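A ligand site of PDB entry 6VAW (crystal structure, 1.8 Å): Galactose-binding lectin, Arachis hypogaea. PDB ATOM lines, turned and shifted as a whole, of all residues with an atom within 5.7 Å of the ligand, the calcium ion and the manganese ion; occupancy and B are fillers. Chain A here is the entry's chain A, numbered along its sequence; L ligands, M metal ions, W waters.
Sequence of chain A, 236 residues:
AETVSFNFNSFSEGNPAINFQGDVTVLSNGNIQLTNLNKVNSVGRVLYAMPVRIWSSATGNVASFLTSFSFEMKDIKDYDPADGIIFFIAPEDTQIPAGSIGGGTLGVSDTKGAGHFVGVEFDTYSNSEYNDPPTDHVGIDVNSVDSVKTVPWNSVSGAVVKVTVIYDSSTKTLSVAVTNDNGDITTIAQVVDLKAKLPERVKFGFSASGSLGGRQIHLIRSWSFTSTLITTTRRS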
ATOM      1  N   ASP A  80      29.258 -37.632 -30.071  1.00  0.00           N
ATOM      2  CA  ASP A  80      29.790 -36.860 -28.945  1.00  0.00           C
ATOM      3  C   ASP A  80      28.675 -36.546 -27.988  1.00  0.00           C
ATOM      4  O   ASP A  80      27.653 -36.073 -28.448  1.00  0.00           O
ATOM      5  CB  ASP A  80      30.391 -35.552 -29.456  1.00  0.00           C
ATOM      6  CG  ASP A  80      31.856 -35.500 -29.201  1.00  0.00           C
ATOM      7  OD1 ASP A  80      32.563 -36.297 -29.814  1.00  0.00           O
ATOM      8  OD2 ASP A  80      32.281 -34.785 -28.272  1.00  0.00           O
ATOM      9  N   ALA A  82      26.519 -34.506 -26.380  1.00  0.00           N
ATOM     10  CA  ALA A  82      26.198 -33.087 -26.502  1.00  0.00           C
ATOM     11  C   ALA A  82      24.693 -32.884 -26.874  1.00  0.00           C
ATOM     12  O   ALA A  82      24.074 -33.835 -27.358  1.00  0.00           O
ATOM     13  CB  ALA A  82      27.116 -32.446 -27.554  1.00  0.00           C
ATOM     14  N   ASP A  83      24.105 -31.696 -26.623  1.00  0.00           N
ATOM     15  CA  ASP A  83      24.817 -30.526 -26.092  1.00  0.00           C
ATOM     16  C   ASP A  83      24.486 -30.125 -24.642  1.00  0.00           C
ATOM     17  O   ASP A  83      25.209 -29.292 -24.092  1.00  0.00           O
ATOM     18  CB  ASP A  83      24.568 -29.339 -26.976  1.00  0.00           C
ATOM     19  CG  ASP A  83      25.515 -29.344 -28.136  1.00  0.00           C
ATOM     20  OD1 ASP A  83      25.186 -29.993 -29.166  1.00  0.00           O
ATOM     21  OD2 ASP A  83      26.637 -28.813 -27.984  1.00  0.00           O
ATOM     22  N   GLY A 103      22.654 -27.553 -31.452  1.00  0.00           N
ATOM     23  CA  GLY A 103      24.012 -27.537 -30.923  1.00  0.00           C
ATOM     24  C   GLY A 103      24.168 -26.752 -29.630  1.00  0.00           C
ATOM     25  O   GLY A 103      23.391 -26.942 -28.683  1.00  0.00           O
ATOM     26  N   GLY A 104      25.150 -25.857 -29.601  1.00  0.00           N
ATOM     27  CA  GLY A 104      25.502 -25.014 -28.465  1.00  0.00           C
ATOM     28  C   GLY A 104      24.464 -23.950 -28.121  1.00  0.00           C
ATOM     29  O   GLY A 104      24.572 -23.316 -27.067  1.00  0.00           O
ATOM     30  N   LEU A 106      21.424 -24.565 -27.482  1.00  0.00           N
ATOM     31  CA  LEU A 106      20.555 -25.298 -26.524  1.00  0.00           C
ATOM     32  C   LEU A 106      19.038 -25.138 -26.838  1.00  0.00           C
ATOM     33  O   LEU A 106      18.194 -25.393 -25.961  1.00  0.00           O
ATOM     34  CB  LEU A 106      20.878 -24.870 -25.061  1.00  0.00           C
ATOM     35  CG  LEU A 106      22.324 -25.066 -24.603  1.00  0.00           C
ATOM     36  CD1 LEU A 106      22.555 -24.424 -23.219  1.00  0.00           C
ATOM     37  CD2 LEU A 106      22.741 -26.555 -24.627  1.00  0.00           C
ATOM     38  N   GLU A 121      21.658 -23.528 -17.410  1.00  0.00           N
ATOM     39  CA  GLU A 121      22.121 -24.549 -18.357  1.00  0.00           C
ATOM     40  C   GLU A 121      23.004 -25.585 -17.693  1.00  0.00           C
ATOM     41  O   GLU A 121      23.793 -25.284 -16.790  1.00  0.00           O
ATOM     42  CB  GLU A 121      22.868 -23.938 -19.546  1.00  0.00           C
ATOM     43  CG  GLU A 121      24.070 -23.099 -19.115  1.00  0.00           C
ATOM     44  CD  GLU A 121      24.951 -22.730 -20.278  1.00  0.00           C
ATOM     45  OE1 GLU A 121      24.460 -21.985 -21.142  1.00  0.00           O
ATOM     46  OE2 GLU A 121      26.130 -23.136 -20.306  1.00  0.00           O
ATOM     47  N   ASP A 123      25.451 -27.718 -19.353  1.00  0.00           N
ATOM     48  CA  ASP A 123      26.190 -27.718 -20.607  1.00  0.00           C
ATOM     49  C   ASP A 123      27.285 -28.770 -20.652  1.00  0.00           C
ATOM     50  O   ASP A 123      28.185 -28.778 -19.820  1.00  0.00           O
ATOM     51  CB  ASP A 123      26.758 -26.318 -20.803  1.00  0.00           C
ATOM     52  CG  ASP A 123      27.163 -26.029 -22.211  1.00  0.00           C
ATOM     53  OD1 ASP A 123      27.170 -26.975 -23.036  1.00  0.00           O
ATOM     54  OD2 ASP A 123      27.423 -24.860 -22.518  1.00  0.00           O
ATOM     55  N   THR A 124      27.195 -29.680 -21.652  1.00  0.00           N
ATOM     56  CA  THR A 124      28.106 -30.819 -21.768  1.00  0.00           C
ATOM     57  C   THR A 124      29.093 -30.720 -22.957  1.00  0.00           C
ATOM     58  O   THR A 124      29.817 -31.686 -23.229  1.00  0.00           O
ATOM     59  CB  THR A 124      27.312 -32.129 -21.833  1.00  0.00           C
ATOM     60  OG1 THR A 124      26.595 -32.211 -23.060  1.00  0.00           O
ATOM     61  CG2 THR A 124      26.347 -32.292 -20.667  1.00  0.00           C
ATOM     62  N   TYR A 125      29.180 -29.540 -23.617  1.00  0.00           N
ATOM     63  CA  TYR A 125      30.098 -29.329 -24.755  1.00  0.00           C
ATOM     64  C   TYR A 125      30.588 -27.880 -24.763  1.00  0.00           C
ATOM     65  O   TYR A 125      29.787 -26.942 -24.690  1.00  0.00           O
ATOM     66  CB  TYR A 125      29.430 -29.710 -26.095  1.00  0.00           C
ATOM     67  CG  TYR A 125      30.406 -29.604 -27.257  1.00  0.00           C
ATOM     68  CD1 TYR A 125      30.625 -28.385 -27.906  1.00  0.00           C
ATOM     69  CD2 TYR A 125      31.147 -30.703 -27.676  1.00  0.00           C
ATOM     70  CE1 TYR A 125      31.582 -28.260 -28.906  1.00  0.00           C
ATOM     71  CE2 TYR A 125      32.067 -30.606 -28.714  1.00  0.00           C
ATOM     72  CZ  TYR A 125      32.275 -29.380 -29.336  1.00  0.00           C
ATOM     73  OH  TYR A 125      33.173 -29.283 -30.368  1.00  0.00           O
ATOM     74  N   SER A 126      31.908 -27.694 -24.892  1.00  0.00           N
ATOM     75  CA  SER A 126      32.535 -26.374 -24.880  1.00  0.00           C
ATOM     76  C   SER A 126      32.537 -25.727 -26.262  1.00  0.00           C
ATOM     77  O   SER A 126      33.307 -26.124 -27.128  1.00  0.00           O
ATOM     78  CB  SER A 126      33.958 -26.464 -24.334  1.00  0.00           C
ATOM     79  OG  SER A 126      34.544 -25.184 -24.221  1.00  0.00           O
ATOM     80  N   ASN A 127      31.645 -24.734 -26.459  1.00  0.00           N
ATOM     81  CA  ASN A 127      31.514 -23.976 -27.695  1.00  0.00           C
ATOM     82  C   ASN A 127      32.335 -22.708 -27.552  1.00  0.00           C
ATOM     83  O   ASN A 127      31.949 -21.801 -26.810  1.00  0.00           O
ATOM     84  CB  ASN A 127      30.053 -23.663 -27.988  1.00  0.00           C
ATOM     85  CG  ASN A 127      29.216 -24.880 -28.188  1.00  0.00           C
ATOM     86  OD1 ASN A 127      28.839 -25.575 -27.238  1.00  0.00           O
ATOM     87  ND2 ASN A 127      28.949 -25.217 -29.430  1.00  0.00           N
ATOM     88  N   GLU A 129      32.707 -20.361 -29.661  1.00  0.00           N
ATOM     89  CA  GLU A 129      31.913 -19.274 -30.255  1.00  0.00           C
ATOM     90  C   GLU A 129      31.008 -18.602 -29.179  1.00  0.00           C
ATOM     91  O   GLU A 129      30.594 -17.454 -29.339  1.00  0.00           O
ATOM     92  CB  GLU A 129      31.089 -19.756 -31.484  1.00  0.00           C
ATOM     93  CG  GLU A 129      30.016 -20.803 -31.198  1.00  0.00           C
ATOM     94  CD  GLU A 129      30.431 -22.262 -31.268  1.00  0.00           C
ATOM     95  OE1 GLU A 129      31.605 -22.586 -30.981  1.00  0.00           O
ATOM     96  OE2 GLU A 129      29.536 -23.097 -31.536  1.00  0.00           O
ATOM     97  N   TYR A 130      30.748 -19.307 -28.063  1.00  0.00           N
ATOM     98  CA  TYR A 130      29.892 -18.812 -26.961  1.00  0.00           C
ATOM     99  C   TYR A 130      30.667 -18.631 -25.673  1.00  0.00           C
ATOM    100  O   TYR A 130      30.059 -18.511 -24.605  1.00  0.00           O
ATOM    101  CB  TYR A 130      28.707 -19.768 -26.745  1.00  0.00           C
ATOM    102  CG  TYR A 130      27.895 -19.994 -27.999  1.00  0.00           C
ATOM    103  CD1 TYR A 130      27.493 -18.921 -28.798  1.00  0.00           C
ATOM    104  CD2 TYR A 130      27.473 -21.268 -28.358  1.00  0.00           C
ATOM    105  CE1 TYR A 130      26.743 -19.123 -29.948  1.00  0.00           C
ATOM    106  CE2 TYR A 130      26.749 -21.483 -29.530  1.00  0.00           C
ATOM    107  CZ  TYR A 130      26.381 -20.406 -30.328  1.00  0.00           C
ATOM    108  OH  TYR A 130      25.642 -20.584 -31.464  1.00  0.00           O
ATOM    109  N   ASP A 132      32.421 -20.686 -23.882  1.00  0.00           N
ATOM    110  CA  ASP A 132      32.183 -21.726 -22.880  1.00  0.00           C
ATOM    111  C   ASP A 132      33.453 -22.026 -22.100  1.00  0.00           C
ATOM    112  O   ASP A 132      34.517 -22.047 -22.707  1.00  0.00           O
ATOM    113  CB  ASP A 132      31.697 -23.023 -23.548  1.00  0.00           C
ATOM    114  CG  ASP A 132      30.191 -23.170 -23.684  1.00  0.00           C
ATOM    115  OD1 ASP A 132      29.458 -22.534 -22.888  1.00  0.00           O
ATOM    116  OD2 ASP A 132      29.748 -23.923 -24.574  1.00  0.00           O
ATOM    117  N   PRO A 133      33.359 -22.377 -20.797  1.00  0.00           N
ATOM    118  CA  PRO A 133      34.578 -22.810 -20.078  1.00  0.00           C
ATOM    119  C   PRO A 133      35.078 -24.163 -20.645  1.00  0.00           C
ATOM    120  O   PRO A 133      34.333 -24.811 -21.379  1.00  0.00           O
ATOM    121  CB  PRO A 133      34.136 -22.894 -18.606  1.00  0.00           C
ATOM    122  CG  PRO A 133      32.661 -23.027 -18.652  1.00  0.00           C
ATOM    123  CD  PRO A 133      32.160 -22.428 -19.927  1.00  0.00           C
ATOM    124  N   HIS A 137      29.703 -27.734 -17.365  1.00  0.00           N
ATOM    125  CA  HIS A 137      29.431 -26.661 -16.424  1.00  0.00           C
ATOM    126  C   HIS A 137      27.951 -26.386 -16.278  1.00  0.00           C
ATOM    127  O   HIS A 137      27.150 -26.724 -17.164  1.00  0.00           O
ATOM    128  CB  HIS A 137      30.137 -25.357 -16.883  1.00  0.00           C
ATOM    129  CG  HIS A 137      29.817 -24.970 -18.292  1.00  0.00           C
ATOM    130  ND1 HIS A 137      30.463 -25.563 -19.384  1.00  0.00           N
ATOM    131  CD2 HIS A 137      28.959 -24.037 -18.764  1.00  0.00           C
ATOM    132  CE1 HIS A 137      29.954 -24.992 -20.459  1.00  0.00           C
ATOM    133  NE2 HIS A 137      29.050 -24.065 -20.140  1.00  0.00           N
ATOM    134  N   VAL A 145      23.552 -17.547 -24.494  1.00  0.00           N
ATOM    135  CA  VAL A 145      24.195 -18.797 -24.098  1.00  0.00           C
ATOM    136  C   VAL A 145      25.687 -18.518 -23.805  1.00  0.00           C
ATOM    137  O   VAL A 145      26.461 -19.440 -23.520  1.00  0.00           O
ATOM    138  CB  VAL A 145      23.983 -19.993 -25.077  1.00  0.00           C
ATOM    139  CG1 VAL A 145      22.531 -20.466 -25.053  1.00  0.00           C
ATOM    140  CG2 VAL A 145      24.427 -19.655 -26.496  1.00  0.00           C
ATOM    141  N   SER A 147      27.138 -17.344 -20.972  1.00  0.00           N
ATOM    142  CA  SER A 147      26.664 -17.201 -19.595  1.00  0.00           C
ATOM    143  C   SER A 147      27.234 -15.998 -18.826  1.00  0.00           C
ATOM    144  O   SER A 147      28.402 -15.629 -18.947  1.00  0.00           O
ATOM    145  CB  SER A 147      26.928 -18.462 -18.799  1.00  0.00           C
ATOM    146  OG  SER A 147      26.431 -19.598 -19.466  1.00  0.00           O
ATOM    147  N   THR A 150      29.356 -19.140 -14.663  1.00  0.00           N
ATOM    148  CA  THR A 150      29.403 -20.597 -14.754  1.00  0.00           C
ATOM    149  C   THR A 150      30.144 -21.166 -13.548  1.00  0.00           C
ATOM    150  O   THR A 150      30.928 -20.466 -12.889  1.00  0.00           O
ATOM    151  CB  THR A 150      30.070 -21.151 -16.059  1.00  0.00           C
ATOM    152  OG1 THR A 150      31.460 -20.865 -16.056  1.00  0.00           O
ATOM    153  CG2 THR A 150      29.389 -20.688 -17.344  1.00  0.00           C
ATOM    154  N   GLY A 210      21.015 -30.954 -30.055  1.00  0.00           N
ATOM    155  CA  GLY A 210      22.172 -31.688 -30.558  1.00  0.00           C
ATOM    156  C   GLY A 210      22.593 -31.101 -31.885  1.00  0.00           C
ATOM    157  O   GLY A 210      22.005 -30.134 -32.370  1.00  0.00           O
ATOM    158  N   SER A 211      23.602 -31.711 -32.494  1.00  0.00           N
ATOM    159  CA  SER A 211      24.137 -31.330 -33.790  1.00  0.00           C
ATOM    160  C   SER A 211      24.298 -32.601 -34.681  1.00  0.00           C
ATOM    161  O   SER A 211      23.792 -33.654 -34.320  1.00  0.00           O
ATOM    162  CB  SER A 211      25.460 -30.597 -33.620  1.00  0.00           C
ATOM    163  OG  SER A 211      26.442 -31.486 -33.101  1.00  0.00           O
ATOM    164  N   LEU A 212      25.041 -32.502 -35.792  1.00  0.00           N
ATOM    165  CA  LEU A 212      25.255 -33.668 -36.641  1.00  0.00           C
ATOM    166  C   LEU A 212      26.038 -34.725 -35.875  1.00  0.00           C
ATOM    167  O   LEU A 212      25.589 -35.865 -35.813  1.00  0.00           O
ATOM    168  CB  LEU A 212      25.965 -33.273 -37.958  1.00  0.00           C
ATOM    169  CG  LEU A 212      26.173 -34.408 -39.003  1.00  0.00           C
ATOM    170  CD1 LEU A 212      25.961 -33.910 -40.430  1.00  0.00           C
ATOM    171  CD2 LEU A 212      27.559 -34.986 -38.882  1.00  0.00           C
ATOM    172  N   GLY A 213      27.191 -34.325 -35.312  1.00  0.00           N
ATOM    173  CA  GLY A 213      28.080 -35.204 -34.556  1.00  0.00           C
ATOM    174  C   GLY A 213      27.885 -35.239 -33.044  1.00  0.00           C
ATOM    175  O   GLY A 213      28.397 -36.141 -32.378  1.00  0.00           O
ATOM    176  N   GLY A 214      27.126 -34.278 -32.514  1.00  0.00           N
ATOM    177  CA  GLY A 214      26.874 -34.199 -31.084  1.00  0.00           C
ATOM    178  C   GLY A 214      25.448 -34.496 -30.733  1.00  0.00           C
ATOM    179  O   GLY A 214      24.547 -33.708 -31.054  1.00  0.00           O
HETATM  180  N1  LIG L   1      29.526 -28.509 -34.530  1.00  0.00           N
HETATM  181  N2  LIG L   1      31.527 -31.334 -38.437  1.00  0.00           N
HETATM  182  C1  LIG L   1      31.173 -32.694 -38.764  1.00  0.00           C
HETATM  183  C2  LIG L   1      28.520 -29.786 -30.618  1.00  0.00           C
HETATM  184  C3  LIG L   1      28.594 -28.284 -30.889  1.00  0.00           C
HETATM  185  C4  LIG L   1      29.540 -30.517 -31.498  1.00  0.00           C
HETATM  186  C5  LIG L   1      29.592 -28.761 -33.124  1.00  0.00           C
HETATM  187  C6  LIG L   1      28.494 -28.000 -32.385  1.00  0.00           C
HETATM  188  C7  LIG L   1      29.772 -31.996 -31.341  1.00  0.00           C
HETATM  189  C8  LIG L   1      30.592 -28.552 -35.338  1.00  0.00           C
HETATM  190  C9  LIG L   1      30.333 -28.222 -36.792  1.00  0.00           C
HETATM  191  C10 LIG L   1      31.167 -29.044 -37.765  1.00  0.00           C
HETATM  192  C11 LIG L   1      30.652 -30.448 -37.954  1.00  0.00           C
HETATM  193  O1  LIG L   1      29.443 -30.166 -32.891  1.00  0.00           O
HETATM  194  O2  LIG L   1      28.639 -26.608 -32.620  1.00  0.00           O
HETATM  195  O3  LIG L   1      27.588 -27.586 -30.174  1.00  0.00           O
HETATM  196  O4  LIG L   1      27.203 -30.266 -30.845  1.00  0.00           O
HETATM  197  O5  LIG L   1      31.118 -32.337 -31.666  1.00  0.00           O
HETATM  198  O6  LIG L   1      29.484 -30.739 -37.705  1.00  0.00           O
HETATM  199  O7  LIG L   1      31.722 -28.804 -34.933  1.00  0.00           O
HETATM  200 CA    CA M   1      28.114 -25.610 -24.874  1.00  0.00          CA
HETATM  201 MN    MN M   2      27.851 -23.087 -21.538  1.00  0.00          MN
HETATM  202  O   HOH W   1      28.805 -31.782 -35.222  1.00  0.00           O
HETATM  203  O   HOH W   2      26.567 -23.823 -25.309  1.00  0.00           O
HETATM  204  O   HOH W   3      26.402 -25.074 -32.281  1.00  0.00           O
HETATM  205  O   HOH W   4      30.965 -25.402 -31.897  1.00  0.00           O
HETATM  206  O   HOH W   5      28.425 -21.094 -20.593  1.00  0.00           O
HETATM  207  O   HOH W   6      26.271 -22.017 -23.137  1.00  0.00           O
HETATM  208  O   HOH W   7      26.640 -27.177 -25.671  1.00  0.00           O
HETATM  209  O   HOH W   8      27.162 -28.040 -35.586  1.00  0.00           O
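OD1 of Asp 83 lies within hydrogen-bond range of O4 of the ligand (2.6 Å).
OG of Ser 211 sits at hydrogen-bond distance from O4 of the ligand (2.7 Å).
The side-chain amide nitrogen of Asn 127 sits at hydrogen-bond distance from an oxygen (O3) of the ligand (2.8 Å).
The backbone NH (N) of Gly 104 is in hydrogen-bond range of an oxygen (O3) of the ligand (3.0 Å).
The manganese ion is bound by OD2 of Asp 123 (2.1 Å), NE2 of His 137 (2.1 Å), OE2 of Glu 121 (2.1 Å), OD1 of Asp 132 (2.2 Å), water W5 (2.3 Å) and water W6 (2.5 Å).
Water W6 lies within hydrogen-bond range of O of Val 145 and OE1 of Glu 121.
Water W4 lies within hydrogen-bond range of O2 of the ligand, OE2 of Glu 129 and ND2 of Asn 127.
Water W3 lies within hydrogen-bond range of an oxygen (O2) of the ligand (2.7 Å) and the backbone NH of Gly 104 (3.1 Å).
Water W1 lies within hydrogen-bond range of an oxygen (O6) of the ligand (2.8 Å), the backbone NH (N) of Gly 213 (3.0 Å) and the side-chain hydroxyl (OG) of Ser 211 (3.2 Å).
The nearest printed residue that does not touch the manganese ion is Ser 147 (4.3 Å).
The nearest printed residue that does not touch the calcium ion is Ser 126 (4.3 Å).
O of Asp 132 sits at hydrogen-bond distance from OG of Ser 126 (3.5 Å).
The backbone carbonyl oxygen of Gly 210 is in hydrogen-bond range of the backbone NH of Gly 103 (2.8 Å).
O of Asp 83 lies within hydrogen-bond range of N of Thr 124 (3.2 Å).
OG of Ser 211 sits at hydrogen-bond distance from N of Gly 214, 2.9 Å away.
OE2 of Glu 129 is in hydrogen-bond range of ND2 of Asn 127, 3.0 Å away.
N of Asp 80 sits at hydrogen-bond distance from O of Gly 213, 2.9 Å away.
The calcium ion is bound by O of Tyr 125 (2.1 Å), water W7 (2.3 Å), OD2 of Asp 132 (2.4 Å), water W2 (2.4 Å), OD1 of Asn 127 (2.5 Å), OD1 of Asp 123 (2.5 Å) and OD2 of Asp 123 (2.6 Å).
The calcium ion has seven donor atoms within binding distance.
Asp 80 touches the ligand.
CB of Ala 82 touches O4 of the ligand, at 3.9 Å.
Gly 103 touches the ligand (C to O3, 3.6 Å).
Glu 129 touches the ligand.
CA of Gly 214 touches C7 of the ligand (3.6 Å).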
